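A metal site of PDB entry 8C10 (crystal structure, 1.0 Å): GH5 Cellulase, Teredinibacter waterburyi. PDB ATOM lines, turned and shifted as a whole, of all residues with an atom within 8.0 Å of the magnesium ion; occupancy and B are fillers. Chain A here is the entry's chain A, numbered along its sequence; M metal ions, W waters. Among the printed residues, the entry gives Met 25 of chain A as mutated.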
ATOM      1  N   MET A  25     -23.912   7.623  33.278  1.00  0.00           N
ATOM      2  CA  MET A  25     -24.596   7.269  32.094  1.00  0.00           C
ATOM      3  C   MET A  25     -25.225   8.467  31.380  1.00  0.00           C
ATOM      4  O   MET A  25     -26.080   9.136  31.964  1.00  0.00           O
ATOM      5  CB  MET A  25     -25.628   6.260  32.408  1.00  0.00           C
ATOM      6  CG  MET A  25     -25.076   4.964  33.250  1.00  0.00           C
ATOM      7  SD  MET A  25     -23.782   4.188  32.411  1.00  0.00           S
ATOM      8  CE  MET A  25     -24.973   3.529  31.601  1.00  0.00           C
ATOM      9  N   ALA A  29     -31.639   5.169  30.027  1.00  0.00           N
ATOM     10  CA  ALA A  29     -31.781   3.696  29.775  1.00  0.00           C
ATOM     11  C   ALA A  29     -33.083   3.417  29.070  1.00  0.00           C
ATOM     12  O   ALA A  29     -34.124   4.043  29.347  1.00  0.00           O
ATOM     13  CB  ALA A  29     -31.732   2.956  31.083  1.00  0.00           C
ATOM     14  N   VAL A  30     -33.045   2.402  28.193  1.00  0.00           N
ATOM     15  CA  VAL A  30     -34.201   1.945  27.474  1.00  0.00           C
ATOM     16  C   VAL A  30     -34.793   0.744  28.191  1.00  0.00           C
ATOM     17  O   VAL A  30     -34.066  -0.184  28.568  1.00  0.00           O
ATOM     18  CB  VAL A  30     -33.851   1.580  26.035  1.00  0.00           C
ATOM     19  CG1 VAL A  30     -35.134   1.374  25.226  1.00  0.00           C
ATOM     20  CG2 VAL A  30     -32.988   2.637  25.366  1.00  0.00           C
ATOM     21  N   ALA A 141     -22.789  -8.097  23.960  1.00  0.00           N
ATOM     22  CA  ALA A 141     -23.217  -7.769  25.323  1.00  0.00           C
ATOM     23  C   ALA A 141     -22.027  -7.559  26.241  1.00  0.00           C
ATOM     24  O   ALA A 141     -22.062  -6.633  27.089  1.00  0.00           O
ATOM     25  CB  ALA A 141     -24.109  -8.857  25.862  1.00  0.00           C
ATOM     26  N   TYR A 144     -20.467  -4.074  25.065  1.00  0.00           N
ATOM     27  CA  TYR A 144     -21.289  -2.880  24.997  1.00  0.00           C
ATOM     28  C   TYR A 144     -22.432  -2.804  25.985  1.00  0.00           C
ATOM     29  O   TYR A 144     -23.082  -1.747  26.055  1.00  0.00           O
ATOM     30  CB  TYR A 144     -21.899  -2.745  23.574  1.00  0.00           C
ATOM     31  CG  TYR A 144     -20.827  -2.476  22.511  1.00  0.00           C
ATOM     32  CD1 TYR A 144     -20.038  -1.327  22.546  1.00  0.00           C
ATOM     33  CD2 TYR A 144     -20.690  -3.329  21.412  1.00  0.00           C
ATOM     34  CE1 TYR A 144     -19.144  -1.072  21.562  1.00  0.00           C
ATOM     35  CE2 TYR A 144     -19.791  -3.043  20.398  1.00  0.00           C
ATOM     36  CZ  TYR A 144     -19.025  -1.903  20.460  1.00  0.00           C
ATOM     37  OH  TYR A 144     -18.153  -1.634  19.431  1.00  0.00           O
ATOM     38  N   GLY A 145     -22.716  -3.861  26.744  1.00  0.00           N
ATOM     39  CA  GLY A 145     -23.952  -3.905  27.517  1.00  0.00           C
ATOM     40  C   GLY A 145     -24.061  -2.967  28.688  1.00  0.00           C
ATOM     41  O   GLY A 145     -25.157  -2.761  29.205  1.00  0.00           O
ATOM     42  N   ASN A 146     -22.959  -2.337  29.083  1.00  0.00           N
ATOM     43  CA  ASN A 146     -23.026  -1.285  30.106  1.00  0.00           C
ATOM     44  C   ASN A 146     -23.234   0.058  29.538  1.00  0.00           C
ATOM     45  O   ASN A 146     -23.278   1.049  30.331  1.00  0.00           O
ATOM     46  CB  ASN A 146     -21.776  -1.291  30.979  1.00  0.00           C
ATOM     47  CG  ASN A 146     -21.930  -2.398  32.031  1.00  0.00           C
ATOM     48  OD1 ASN A 146     -23.083  -2.620  32.569  1.00  0.00           O
ATOM     49  ND2 ASN A 146     -20.872  -3.066  32.308  1.00  0.00           N
ATOM     50  N   ASN A 147     -23.429   0.220  28.242  1.00  0.00           N
ATOM     51  CA  ASN A 147     -23.802   1.482  27.671  1.00  0.00           C
ATOM     52  C   ASN A 147     -25.305   1.571  27.458  1.00  0.00           C
ATOM     53  O   ASN A 147     -25.886   0.673  26.824  1.00  0.00           O
ATOM     54  CB  ASN A 147     -23.132   1.703  26.278  1.00  0.00           C
ATOM     55  CG  ASN A 147     -21.651   1.733  26.372  1.00  0.00           C
ATOM     56  OD1 ASN A 147     -21.056   2.744  26.762  1.00  0.00           O
ATOM     57  ND2 ASN A 147     -21.012   0.651  26.052  1.00  0.00           N
ATOM     58  N   ASN A 148     -25.965   2.628  27.937  1.00  0.00           N
ATOM     59  CA  ASN A 148     -27.422   2.732  27.733  1.00  0.00           C
ATOM     60  C   ASN A 148     -27.799   2.903  26.270  1.00  0.00           C
ATOM     61  O   ASN A 148     -28.954   2.719  25.906  1.00  0.00           O
ATOM     62  CB  ASN A 148     -27.972   3.878  28.565  1.00  0.00           C
ATOM     63  CG  ASN A 148     -28.096   3.579  30.072  1.00  0.00           C
ATOM     64  OD1 ASN A 148     -28.050   2.423  30.482  1.00  0.00           O
ATOM     65  ND2 ASN A 148     -28.336   4.632  30.852  1.00  0.00           N
ATOM     66  N   VAL A 150     -27.092   1.078  23.683  1.00  0.00           N
ATOM     67  CA  VAL A 150     -27.097  -0.095  22.816  1.00  0.00           C
ATOM     68  C   VAL A 150     -28.357  -0.908  22.959  1.00  0.00           C
ATOM     69  O   VAL A 150     -28.786  -1.252  24.067  1.00  0.00           O
ATOM     70  CB  VAL A 150     -25.814  -0.909  23.091  1.00  0.00           C
ATOM     71  CG1 VAL A 150     -25.841  -2.246  22.350  1.00  0.00           C
ATOM     72  CG2 VAL A 150     -24.593  -0.079  22.731  1.00  0.00           C
ATOM     73  N   TYR A 152     -30.338  -4.395  21.107  1.00  0.00           N
ATOM     74  CA  TYR A 152     -30.090  -5.589  20.293  1.00  0.00           C
ATOM     75  C   TYR A 152     -31.335  -5.940  19.482  1.00  0.00           C
ATOM     76  O   TYR A 152     -32.413  -6.021  20.053  1.00  0.00           O
ATOM     77  CB  TYR A 152     -29.746  -6.784  21.179  1.00  0.00           C
ATOM     78  CG  TYR A 152     -28.644  -6.489  22.202  1.00  0.00           C
ATOM     79  CD1 TYR A 152     -27.330  -6.366  21.860  1.00  0.00           C
ATOM     80  CD2 TYR A 152     -28.998  -6.309  23.542  1.00  0.00           C
ATOM     81  CE1 TYR A 152     -26.349  -6.103  22.799  1.00  0.00           C
ATOM     82  CE2 TYR A 152     -28.034  -6.045  24.496  1.00  0.00           C
ATOM     83  CZ  TYR A 152     -26.713  -5.923  24.142  1.00  0.00           C
ATOM     84  OH  TYR A 152     -25.727  -5.680  25.067  1.00  0.00           O
ATOM     85  N   ILE A 178     -28.044 -13.309  26.174  1.00  0.00           N
ATOM     86  CA  ILE A 178     -27.764 -11.890  26.383  1.00  0.00           C
ATOM     87  C   ILE A 178     -27.983 -11.500  27.830  1.00  0.00           C
ATOM     88  O   ILE A 178     -27.140 -10.821  28.435  1.00  0.00           O
ATOM     89  CB  ILE A 178     -28.629 -11.008  25.458  1.00  0.00           C
ATOM     90  CG1 ILE A 178     -28.207 -11.199  23.993  1.00  0.00           C
ATOM     91  CG2 ILE A 178     -28.493  -9.553  25.845  1.00  0.00           C
ATOM     92  CD1 ILE A 178     -29.178 -10.563  23.003  1.00  0.00           C
ATOM     93  N   ARG A 179     -29.115 -11.907  28.398  1.00  0.00           N
ATOM     94  CA  ARG A 179     -29.540 -11.467  29.729  1.00  0.00           C
ATOM     95  C   ARG A 179     -28.614 -11.961  30.806  1.00  0.00           C
ATOM     96  O   ARG A 179     -28.513 -11.293  31.854  1.00  0.00           O
ATOM     97  CB  ARG A 179     -30.988 -11.873  29.989  1.00  0.00           C
ATOM     98  CG  ARG A 179     -32.027 -11.010  29.234  1.00  0.00           C
ATOM     99  CD  ARG A 179     -32.311  -9.739  30.003  1.00  0.00           C
ATOM    100  NE  ARG A 179     -33.168  -8.820  29.318  1.00  0.00           N
ATOM    101  CZ  ARG A 179     -32.766  -7.805  28.512  1.00  0.00           C
ATOM    102  NH1 ARG A 179     -31.483  -7.518  28.371  1.00  0.00           N
ATOM    103  NH2 ARG A 179     -33.664  -7.134  27.838  1.00  0.00           N
ATOM    104  N   ILE A 181     -25.538 -11.797  30.701  1.00  0.00           N
ATOM    105  CA  ILE A 181     -24.454 -10.820  30.693  1.00  0.00           C
ATOM    106  C   ILE A 181     -24.947  -9.426  30.905  1.00  0.00           C
ATOM    107  O   ILE A 181     -24.320  -8.618  31.623  1.00  0.00           O
ATOM    108  CB  ILE A 181     -23.668 -10.906  29.334  1.00  0.00           C
ATOM    109  CG1 ILE A 181     -23.040 -12.299  29.190  1.00  0.00           C
ATOM    110  CG2 ILE A 181     -22.652  -9.804  29.189  1.00  0.00           C
ATOM    111  CD1 ILE A 181     -22.727 -12.620  27.754  1.00  0.00           C
ATOM    112  N   ASP A 182     -26.034  -9.066  30.225  1.00  0.00           N
ATOM    113  CA  ASP A 182     -26.554  -7.692  30.131  1.00  0.00           C
ATOM    114  C   ASP A 182     -28.022  -7.771  30.539  1.00  0.00           C
ATOM    115  O   ASP A 182     -28.902  -8.102  29.723  1.00  0.00           O
ATOM    116  CB  ASP A 182     -26.404  -7.159  28.709  1.00  0.00           C
ATOM    117  CG  ASP A 182     -26.837  -5.712  28.565  1.00  0.00           C
ATOM    118  OD1 ASP A 182     -27.159  -5.118  29.620  1.00  0.00           O
ATOM    119  OD2 ASP A 182     -26.819  -5.210  27.427  1.00  0.00           O
ATOM    120  N   PRO A 183     -28.331  -7.503  31.823  1.00  0.00           N
ATOM    121  CA  PRO A 183     -29.675  -7.782  32.335  1.00  0.00           C
ATOM    122  C   PRO A 183     -30.753  -6.811  31.882  1.00  0.00           C
ATOM    123  O   PRO A 183     -31.933  -7.129  32.024  1.00  0.00           O
ATOM    124  CB  PRO A 183     -29.514  -7.681  33.861  1.00  0.00           C
ATOM    125  CG  PRO A 183     -28.360  -6.742  34.038  1.00  0.00           C
ATOM    126  CD  PRO A 183     -27.401  -7.121  32.910  1.00  0.00           C
ATOM    127  N   ASP A 184     -30.346  -5.640  31.369  1.00  0.00           N
ATOM    128  CA  ASP A 184     -31.303  -4.556  31.194  1.00  0.00           C
ATOM    129  C   ASP A 184     -31.519  -4.102  29.762  1.00  0.00           C
ATOM    130  O   ASP A 184     -32.652  -3.764  29.405  1.00  0.00           O
ATOM    131  CB  ASP A 184     -30.951  -3.343  32.094  1.00  0.00           C
ATOM    132  CG  ASP A 184     -29.487  -2.844  31.931  1.00  0.00           C
ATOM    133  OD1 ASP A 184     -28.679  -3.513  31.256  1.00  0.00           O
ATOM    134  OD2 ASP A 184     -29.204  -1.779  32.526  1.00  0.00           O
ATOM    135  N   ASN A 185     -30.480  -4.032  28.909  1.00  0.00           N
ATOM    136  CA  ASN A 185     -30.659  -3.329  27.634  1.00  0.00           C
ATOM    137  C   ASN A 185     -31.712  -3.982  26.797  1.00  0.00           C
ATOM    138  O   ASN A 185     -31.905  -5.199  26.789  1.00  0.00           O
ATOM    139  CB  ASN A 185     -29.319  -3.297  26.862  1.00  0.00           C
ATOM    140  CG  ASN A 185     -28.287  -2.387  27.466  1.00  0.00           C
ATOM    141  OD1 ASN A 185     -27.643  -1.600  26.668  1.00  0.00           O
ATOM    142  ND2 ASN A 185     -28.060  -2.399  28.714  1.00  0.00           N
ATOM    143  N   LEU A 186     -32.439  -3.134  26.039  1.00  0.00           N
ATOM    144  CA  LEU A 186     -33.550  -3.590  25.224  1.00  0.00           C
ATOM    145  C   LEU A 186     -33.124  -4.630  24.175  1.00  0.00           C
ATOM    146  O   LEU A 186     -32.134  -4.452  23.481  1.00  0.00           O
ATOM    147  CB  LEU A 186     -34.148  -2.376  24.502  1.00  0.00           C
ATOM    148  CG  LEU A 186     -35.398  -2.643  23.648  1.00  0.00           C
ATOM    149  CD1 LEU A 186     -36.558  -2.992  24.500  1.00  0.00           C
ATOM    150  CD2 LEU A 186     -35.737  -1.468  22.748  1.00  0.00           C
HETATM  151 MG    MG M   1     -26.908  -3.184  30.245  1.00  0.00          MG
HETATM  152  O   HOH W   1     -25.697  -3.917  31.785  1.00  0.00           O
HETATM  153  O   HOH W   2     -26.894  -1.331  31.168  1.00  0.00           O
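The backbone carbonyl oxygen of Asn 185 is in hydrogen-bond range of the guanidinium group of Arg 179 (2.8 Å). The side-chain amide oxygen (OD1) of Asn 185 sits close to the backbone carbonyl oxygen (O) of Asn 147, 2.9 Å away. NH1 of Arg 179 lies within hydrogen-bond range of O of Asp 182. OD1 of Asn 185 sits close to O of Val 150 (2.9 Å). OD2 of Asp 182 is in hydrogen-bond range of OH of Tyr 152, 2.6 Å away.
Of the 19 residues printed, 4 come within 4 Å of the magnesium ion. The nearest printed residue that does not touch the magnesium ion is Asn 146 (4.2 Å).
The magnesium ion is bound by OD1 of Asp 182 (2.0 Å), OD1 of Asp 184 (2.1 Å), water W2 (2.1 Å), ND2 of Asn 185 (2.1 Å), O of Gly 145 (2.1 Å) and water W1 (2.1 Å).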
